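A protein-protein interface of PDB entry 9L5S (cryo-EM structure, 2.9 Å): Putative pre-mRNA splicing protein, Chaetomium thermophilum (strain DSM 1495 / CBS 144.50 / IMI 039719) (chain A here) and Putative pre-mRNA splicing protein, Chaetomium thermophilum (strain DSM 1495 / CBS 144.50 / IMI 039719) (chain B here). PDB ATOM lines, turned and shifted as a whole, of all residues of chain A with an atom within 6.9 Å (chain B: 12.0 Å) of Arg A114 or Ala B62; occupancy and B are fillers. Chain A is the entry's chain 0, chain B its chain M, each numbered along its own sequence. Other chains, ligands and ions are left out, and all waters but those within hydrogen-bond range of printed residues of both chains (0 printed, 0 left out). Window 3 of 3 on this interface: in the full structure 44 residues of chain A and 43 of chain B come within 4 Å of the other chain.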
ATOM      1  N   ARG A 110      15.200  26.899  27.880  1.00  0.00           N
ATOM      2  CA  ARG A 110      16.241  26.422  26.977  1.00  0.00           C
ATOM      3  C   ARG A 110      15.978  26.916  25.558  1.00  0.00           C
ATOM      4  O   ARG A 110      16.018  26.136  24.601  1.00  0.00           O
ATOM      5  CB  ARG A 110      16.324  24.894  27.003  1.00  0.00           C
ATOM      6  CG  ARG A 110      17.224  24.343  28.093  1.00  0.00           C
ATOM      7  CD  ARG A 110      17.408  22.842  27.951  1.00  0.00           C
ATOM      8  NE  ARG A 110      16.227  22.100  28.375  1.00  0.00           N
ATOM      9  CZ  ARG A 110      15.383  21.497  27.549  1.00  0.00           C
ATOM     10  NH1 ARG A 110      15.556  21.529  26.239  1.00  0.00           N
ATOM     11  NH2 ARG A 110      14.340  20.844  28.051  1.00  0.00           N
ATOM     12  N   ALA A 111      15.708  28.214  25.420  1.00  0.00           N
ATOM     13  CA  ALA A 111      15.494  28.849  24.125  1.00  0.00           C
ATOM     14  C   ALA A 111      16.199  30.188  23.971  1.00  0.00           C
ATOM     15  O   ALA A 111      16.365  30.639  22.833  1.00  0.00           O
ATOM     16  CB  ALA A 111      13.996  29.045  23.864  1.00  0.00           C
ATOM     17  N   ASP A 112      16.601  30.853  25.058  1.00  0.00           N
ATOM     18  CA  ASP A 112      17.370  32.087  24.933  1.00  0.00           C
ATOM     19  C   ASP A 112      18.780  31.820  24.423  1.00  0.00           C
ATOM     20  O   ASP A 112      19.408  32.710  23.839  1.00  0.00           O
ATOM     21  CB  ASP A 112      17.423  32.815  26.276  1.00  0.00           C
ATOM     22  CG  ASP A 112      16.206  33.688  26.516  1.00  0.00           C
ATOM     23  OD1 ASP A 112      15.813  34.429  25.591  1.00  0.00           O
ATOM     24  OD2 ASP A 112      15.643  33.634  27.630  1.00  0.00           O
ATOM     25  N   SER A 113      19.292  30.606  24.638  1.00  0.00           N
ATOM     26  CA  SER A 113      20.601  30.240  24.114  1.00  0.00           C
ATOM     27  C   SER A 113      20.573  30.000  22.611  1.00  0.00           C
ATOM     28  O   SER A 113      21.603  30.168  21.950  1.00  0.00           O
ATOM     29  CB  SER A 113      21.118  28.993  24.830  1.00  0.00           C
ATOM     30  OG  SER A 113      20.295  27.872  24.553  1.00  0.00           O
ATOM     31  N   ARG A 114      19.422  29.611  22.060  1.00  0.00           N
ATOM     32  CA  ARG A 114      19.306  29.323  20.640  1.00  0.00           C
ATOM     33  C   ARG A 114      18.693  30.515  19.927  1.00  0.00           C
ATOM     34  O   ARG A 114      17.569  30.912  20.271  1.00  0.00           O
ATOM     35  CB  ARG A 114      18.446  28.087  20.416  1.00  0.00           C
ATOM     36  CG  ARG A 114      18.661  26.975  21.426  1.00  0.00           C
ATOM     37  CD  ARG A 114      17.809  25.779  21.063  1.00  0.00           C
ATOM     38  NE  ARG A 114      17.443  24.965  22.217  1.00  0.00           N
ATOM     39  CZ  ARG A 114      18.135  23.919  22.648  1.00  0.00           C
ATOM     40  NH1 ARG A 114      19.247  23.531  22.048  1.00  0.00           N
ATOM     41  NH2 ARG A 114      17.696  23.243  23.706  1.00  0.00           N
ATOM     42  N   PRO A 115      19.372  31.120  18.950  1.00  0.00           N
ATOM     43  CA  PRO A 115      18.736  32.176  18.145  1.00  0.00           C
ATOM     44  C   PRO A 115      17.649  31.585  17.258  1.00  0.00           C
ATOM     45  O   PRO A 115      17.754  30.441  16.810  1.00  0.00           O
ATOM     46  CB  PRO A 115      19.898  32.741  17.318  1.00  0.00           C
ATOM     47  CG  PRO A 115      20.917  31.658  17.289  1.00  0.00           C
ATOM     48  CD  PRO A 115      20.767  30.870  18.553  1.00  0.00           C
ATOM     49  N   GLY A 116      16.605  32.360  17.010  1.00  0.00           N
ATOM     50  CA  GLY A 116      15.525  31.952  16.145  1.00  0.00           C
ATOM     51  C   GLY A 116      14.442  31.089  16.775  1.00  0.00           C
ATOM     52  O   GLY A 116      13.584  30.579  16.042  1.00  0.00           O
ATOM     53  N   SER A 117      14.454  30.908  18.092  1.00  0.00           N
ATOM     54  CA  SER A 117      13.449  30.099  18.767  1.00  0.00           C
ATOM     55  C   SER A 117      12.127  30.850  18.835  1.00  0.00           C
ATOM     56  O   SER A 117      12.094  32.053  19.111  1.00  0.00           O
ATOM     57  CB  SER A 117      13.913  29.727  20.176  1.00  0.00           C
ATOM     58  OG  SER A 117      15.169  29.072  20.142  1.00  0.00           O
ATOM     59  N   TYR A 118      11.037  30.131  18.580  1.00  0.00           N
ATOM     60  CA  TYR A 118       9.714  30.731  18.606  1.00  0.00           C
ATOM     61  C   TYR A 118       9.203  30.860  20.037  1.00  0.00           C
ATOM     62  O   TYR A 118       9.739  30.268  20.978  1.00  0.00           O
ATOM     63  CB  TYR A 118       8.726  29.903  17.783  1.00  0.00           C
ATOM     64  CG  TYR A 118       9.047  29.830  16.309  1.00  0.00           C
ATOM     65  CD1 TYR A 118       8.864  30.932  15.484  1.00  0.00           C
ATOM     66  CD2 TYR A 118       9.526  28.657  15.740  1.00  0.00           C
ATOM     67  CE1 TYR A 118       9.153  30.868  14.136  1.00  0.00           C
ATOM     68  CE2 TYR A 118       9.817  28.585  14.394  1.00  0.00           C
ATOM     69  CZ  TYR A 118       9.629  29.693  13.596  1.00  0.00           C
ATOM     70  OH  TYR A 118       9.919  29.624  12.254  1.00  0.00           O
ATOM     71  N   CYS A 134      11.374  24.157  29.023  1.00  0.00           N
ATOM     72  CA  CYS A 134      10.676  24.280  27.751  1.00  0.00           C
ATOM     73  C   CYS A 134      11.650  24.669  26.646  1.00  0.00           C
ATOM     74  O   CYS A 134      12.606  25.416  26.871  1.00  0.00           O
ATOM     75  CB  CYS A 134       9.557  25.315  27.855  1.00  0.00           C
ATOM     76  SG  CYS A 134       8.288  25.171  26.576  1.00  0.00           S
ATOM     77  N   ASP A 135      11.407  24.149  25.447  1.00  0.00           N
ATOM     78  CA  ASP A 135      12.256  24.439  24.301  1.00  0.00           C
ATOM     79  C   ASP A 135      11.901  25.750  23.611  1.00  0.00           C
ATOM     80  O   ASP A 135      12.610  26.151  22.682  1.00  0.00           O
ATOM     81  CB  ASP A 135      12.182  23.291  23.292  1.00  0.00           C
ATOM     82  CG  ASP A 135      12.737  21.994  23.842  1.00  0.00           C
ATOM     83  OD1 ASP A 135      13.968  21.903  24.029  1.00  0.00           O
ATOM     84  OD2 ASP A 135      11.941  21.061  24.086  1.00  0.00           O
ATOM     85  N   LEU A 137      10.474  30.029  23.953  1.00  0.00           N
ATOM     86  CA  LEU A 137      10.621  31.204  24.799  1.00  0.00           C
ATOM     87  C   LEU A 137       9.404  31.396  25.697  1.00  0.00           C
ATOM     88  O   LEU A 137       8.266  31.157  25.288  1.00  0.00           O
ATOM     89  CB  LEU A 137      10.833  32.451  23.941  1.00  0.00           C
ATOM     90  CG  LEU A 137      12.204  32.597  23.281  1.00  0.00           C
ATOM     91  CD1 LEU A 137      12.244  33.830  22.396  1.00  0.00           C
ATOM     92  CD2 LEU A 137      13.285  32.666  24.343  1.00  0.00           C
ATOM     93  N   PRO B  28      20.809  28.950   5.420  1.00  0.00           N
ATOM     94  CA  PRO B  28      21.680  29.012   6.600  1.00  0.00           C
ATOM     95  C   PRO B  28      22.854  29.963   6.409  1.00  0.00           C
ATOM     96  O   PRO B  28      23.283  30.242   5.287  1.00  0.00           O
ATOM     97  CB  PRO B  28      22.163  27.567   6.757  1.00  0.00           C
ATOM     98  CG  PRO B  28      21.082  26.755   6.166  1.00  0.00           C
ATOM     99  CD  PRO B  28      20.570  27.556   5.003  1.00  0.00           C
ATOM    100  N   GLU B  29      23.362  30.472   7.536  1.00  0.00           N
ATOM    101  CA  GLU B  29      24.549  31.320   7.513  1.00  0.00           C
ATOM    102  C   GLU B  29      25.777  30.552   7.044  1.00  0.00           C
ATOM    103  O   GLU B  29      26.705  31.148   6.484  1.00  0.00           O
ATOM    104  CB  GLU B  29      24.799  31.911   8.901  1.00  0.00           C
ATOM    105  CG  GLU B  29      24.044  33.195   9.178  1.00  0.00           C
ATOM    106  CD  GLU B  29      24.202  33.657  10.612  1.00  0.00           C
ATOM    107  OE1 GLU B  29      25.354  33.749  11.086  1.00  0.00           O
ATOM    108  OE2 GLU B  29      23.174  33.928  11.265  1.00  0.00           O
ATOM    109  N   LYS B  34      23.424  21.507   3.975  1.00  0.00           N
ATOM    110  CA  LYS B  34      22.947  20.134   3.913  1.00  0.00           C
ATOM    111  C   LYS B  34      21.431  20.171   3.756  1.00  0.00           C
ATOM    112  O   LYS B  34      20.724  20.679   4.633  1.00  0.00           O
ATOM    113  CB  LYS B  34      23.353  19.363   5.164  1.00  0.00           C
ATOM    114  CG  LYS B  34      24.854  19.218   5.331  1.00  0.00           C
ATOM    115  CD  LYS B  34      25.192  18.192   6.392  1.00  0.00           C
ATOM    116  CE  LYS B  34      24.788  18.682   7.771  1.00  0.00           C
ATOM    117  NZ  LYS B  34      25.419  17.880   8.852  1.00  0.00           N
ATOM    118  N   TRP B  56      15.904  22.189   5.138  1.00  0.00           N
ATOM    119  CA  TRP B  56      17.238  22.368   5.689  1.00  0.00           C
ATOM    120  C   TRP B  56      17.110  22.828   7.132  1.00  0.00           C
ATOM    121  O   TRP B  56      16.060  23.311   7.561  1.00  0.00           O
ATOM    122  CB  TRP B  56      18.052  23.379   4.873  1.00  0.00           C
ATOM    123  CG  TRP B  56      17.395  24.714   4.793  1.00  0.00           C
ATOM    124  CD1 TRP B  56      17.605  25.780   5.615  1.00  0.00           C
ATOM    125  CD2 TRP B  56      16.403  25.126   3.847  1.00  0.00           C
ATOM    126  NE1 TRP B  56      16.812  26.833   5.237  1.00  0.00           N
ATOM    127  CE2 TRP B  56      16.063  26.456   4.154  1.00  0.00           C
ATOM    128  CE3 TRP B  56      15.773  24.498   2.769  1.00  0.00           C
ATOM    129  CZ2 TRP B  56      15.120  27.169   3.423  1.00  0.00           C
ATOM    130  CZ3 TRP B  56      14.837  25.208   2.046  1.00  0.00           C
ATOM    131  CH2 TRP B  56      14.520  26.528   2.376  1.00  0.00           C
ATOM    132  N   ALA B  57      18.201  22.689   7.876  1.00  0.00           N
ATOM    133  CA  ALA B  57      18.247  23.084   9.276  1.00  0.00           C
ATOM    134  C   ALA B  57      18.795  24.499   9.381  1.00  0.00           C
ATOM    135  O   ALA B  57      19.857  24.802   8.825  1.00  0.00           O
ATOM    136  CB  ALA B  57      19.108  22.119  10.091  1.00  0.00           C
ATOM    137  N   GLY B  58      18.075  25.354  10.096  1.00  0.00           N
ATOM    138  CA  GLY B  58      18.457  26.744  10.219  1.00  0.00           C
ATOM    139  C   GLY B  58      19.662  26.948  11.118  1.00  0.00           C
ATOM    140  O   GLY B  58      20.263  26.014  11.650  1.00  0.00           O
ATOM    141  N   ASP B  59      20.024  28.221  11.279  1.00  0.00           N
ATOM    142  CA  ASP B  59      21.129  28.597  12.153  1.00  0.00           C
ATOM    143  C   ASP B  59      20.801  28.418  13.629  1.00  0.00           C
ATOM    144  O   ASP B  59      21.710  28.491  14.463  1.00  0.00           O
ATOM    145  CB  ASP B  59      21.537  30.041  11.869  1.00  0.00           C
ATOM    146  CG  ASP B  59      21.656  30.323  10.388  1.00  0.00           C
ATOM    147  OD1 ASP B  59      22.538  29.719   9.743  1.00  0.00           O
ATOM    148  OD2 ASP B  59      20.867  31.139   9.867  1.00  0.00           O
ATOM    149  N   GLY B  60      19.535  28.186  13.968  1.00  0.00           N
ATOM    150  CA  GLY B  60      19.143  27.868  15.325  1.00  0.00           C
ATOM    151  C   GLY B  60      19.406  26.410  15.630  1.00  0.00           C
ATOM    152  O   GLY B  60      18.492  25.583  15.585  1.00  0.00           O
ATOM    153  N   ARG B  61      20.673  26.086  15.878  1.00  0.00           N
ATOM    154  CA  ARG B  61      21.095  24.710  16.106  1.00  0.00           C
ATOM    155  C   ARG B  61      20.427  24.107  17.340  1.00  0.00           C
ATOM    156  O   ARG B  61      20.178  24.802  18.331  1.00  0.00           O
ATOM    157  CB  ARG B  61      22.624  24.666  16.232  1.00  0.00           C
ATOM    158  CG  ARG B  61      23.215  23.385  16.814  1.00  0.00           C
ATOM    159  CD  ARG B  61      23.705  22.416  15.750  1.00  0.00           C
ATOM    160  NE  ARG B  61      22.631  21.560  15.260  1.00  0.00           N
ATOM    161  CZ  ARG B  61      22.780  20.624  14.333  1.00  0.00           C
ATOM    162  NH1 ARG B  61      23.957  20.375  13.786  1.00  0.00           N
ATOM    163  NH2 ARG B  61      21.722  19.916  13.950  1.00  0.00           N
ATOM    164  N   ALA B  62      20.065  22.824  17.215  1.00  0.00           N
ATOM    165  CA  ALA B  62      19.678  21.879  18.263  1.00  0.00           C
ATOM    166  C   ALA B  62      18.249  22.042  18.772  1.00  0.00           C
ATOM    167  O   ALA B  62      17.783  21.189  19.536  1.00  0.00           O
ATOM    168  CB  ALA B  62      20.660  21.928  19.441  1.00  0.00           C
ATOM    169  N   HIS B  63      17.544  23.091  18.342  1.00  0.00           N
ATOM    170  CA  HIS B  63      16.082  23.154  18.403  1.00  0.00           C
ATOM    171  C   HIS B  63      15.623  24.334  17.557  1.00  0.00           C
ATOM    172  O   HIS B  63      16.345  25.318  17.380  1.00  0.00           O
ATOM    173  CB  HIS B  63      15.526  23.281  19.830  1.00  0.00           C
ATOM    174  CG  HIS B  63      14.052  23.034  19.922  1.00  0.00           C
ATOM    175  ND1 HIS B  63      13.113  24.025  19.731  1.00  0.00           N
ATOM    176  CD2 HIS B  63      13.355  21.896  20.150  1.00  0.00           C
ATOM    177  CE1 HIS B  63      11.903  23.511  19.847  1.00  0.00           C
ATOM    178  NE2 HIS B  63      12.021  22.222  20.106  1.00  0.00           N
ATOM    179  N   GLY B  64      14.393  24.232  17.068  1.00  0.00           N
ATOM    180  CA  GLY B  64      13.784  25.270  16.265  1.00  0.00           C
ATOM    181  C   GLY B  64      12.758  24.691  15.318  1.00  0.00           C
ATOM    182  O   GLY B  64      11.922  23.876  15.723  1.00  0.00           O
ATOM    183  N   ARG B  65      12.812  25.095  14.054  1.00  0.00           N
ATOM    184  CA  ARG B  65      11.918  24.571  13.034  1.00  0.00           C
ATOM    185  C   ARG B  65      12.723  24.214  11.796  1.00  0.00           C
ATOM    186  O   ARG B  65      13.577  24.989  11.356  1.00  0.00           O
ATOM    187  CB  ARG B  65      10.814  25.580  12.686  1.00  0.00           C
ATOM    188  CG  ARG B  65       9.837  25.151  11.587  1.00  0.00           C
ATOM    189  CD  ARG B  65       8.884  24.029  12.005  1.00  0.00           C
ATOM    190  NE  ARG B  65       9.461  22.701  11.822  1.00  0.00           N
ATOM    191  CZ  ARG B  65       8.906  21.576  12.251  1.00  0.00           C
ATOM    192  NH1 ARG B  65       7.745  21.575  12.885  1.00  0.00           N
ATOM    193  NH2 ARG B  65       9.530  20.422  12.034  1.00  0.00           N
ATOM    194  N   LYS B  66      12.451  23.033  11.248  1.00  0.00           N
ATOM    195  CA  LYS B  66      13.049  22.617   9.984  1.00  0.00           C
ATOM    196  C   LYS B  66      12.490  23.493   8.871  1.00  0.00           C
ATOM    197  O   LYS B  66      11.346  23.307   8.443  1.00  0.00           O
ATOM    198  CB  LYS B  66      12.744  21.142   9.731  1.00  0.00           C
ATOM    199  CG  LYS B  66      13.334  20.569   8.455  1.00  0.00           C
ATOM    200  CD  LYS B  66      14.844  20.447   8.538  1.00  0.00           C
ATOM    201  CE  LYS B  66      15.259  19.321   9.470  1.00  0.00           C
ATOM    202  NZ  LYS B  66      16.736  19.128   9.485  1.00  0.00           N
ATOM    203  N   LYS B  67      13.286  24.458   8.411  1.00  0.00           N
ATOM    204  CA  LYS B  67      12.826  25.363   7.366  1.00  0.00           C
ATOM    205  C   LYS B  67      12.715  24.621   6.042  1.00  0.00           C
ATOM    206  O   LYS B  67      13.511  23.727   5.744  1.00  0.00           O
ATOM    207  CB  LYS B  67      13.774  26.555   7.232  1.00  0.00           C
ATOM    208  CG  LYS B  67      13.890  27.394   8.494  1.00  0.00           C
ATOM    209  CD  LYS B  67      15.017  28.408   8.392  1.00  0.00           C
ATOM    210  CE  LYS B  67      14.557  29.683   7.705  1.00  0.00           C
ATOM    211  NZ  LYS B  67      13.687  30.507   8.590  1.00  0.00           N
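Of chain B, only Arg B61 (3.7 Å), Ala B62 (3.4 Å) and His B63 (3.5 Å) come within 4 Å of Arg A114. Ala B62 touches just one residue of chain A: Arg A114 (3.4 Å). No residue of chain B comes within 4 Å of Ala A111. No residue of chain B comes within 4 Å of Ser A113. Pro A115 touches just one residue of chain B: Gly B60 (3.3 Å). No residue of chain B comes within 4 Å of Gly A116. No residue of chain B comes within 4 Å of Ser A117. Of the printed residues of chain A, Arg B61 touches Arg A114 (3.7 Å). Printed residues of chain A within 4 Å of His B63: Arg A114 and Asp A135. Gly B58 touches none of the printed residues of chain A. Leu A137 touches none of the printed residues of chain B. The nearest residue of chain B that does not touch Arg A114 is Gly B60 (5.1 Å). The nearest residue of chain A that does not touch Ala B62 is Asp A135 (5.9 Å). The nearest printed residue of chain A that does not touch His B63 is Ser A117 (4.8 Å).
O of Arg A110 is in hydrogen-bond range of NE of Arg A114 (3.0 Å). NH1 of Arg A110 lies within salt-bridge range of OD1 of Asp A135, 2.7 Å away. The backbone carbonyl oxygen (O) of Arg A114 sits at hydrogen-bond distance from the side-chain hydroxyl (OG) of Ser A117, 3.0 Å away. NH2 of Arg A114 lies within salt-bridge range of OD1 of Asp A135 (3.97 Å). The backbone carbonyl oxygen (O) of Tyr A118 lies within hydrogen-bond range of the backbone NH (N) of Leu A137 (3.1 Å).
Of the 12 printed residues of chain A, 4 touch a printed residue of chain B. Printed residues of chain A that touch a printed residue of chain B: Arg A114, Pro A115, Tyr A118 and Asp A135. Hydrophobic or aromatic side chains of chain A that line the printed part of chain B: Tyr A118. Of the 15 printed residues of chain B, 5 touch a printed residue of chain A. Printed residues of chain B that touch a printed residue of chain A: Gly B60, Arg B61, Ala B62, His B63 and Arg B65. Among the printed residues, 6 pairs touch across the chains. Among the printed residues, no Asp or Glu carboxylate lies within 4 Å of a Lys or Arg side-chain nitrogen of the other chain.
Among the printed residues, pairs that only touch across the chains: Arg A114 with Arg B61 (3.7 Å), Arg A114 with Ala B62 (3.4 Å), Arg A114 with His B63 (3.5 Å), Pro A115 with Gly B60 (3.3 Å), Tyr A118 with Arg B65 (3.6 Å) and Asp A135 with His B63 (3.4 Å).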
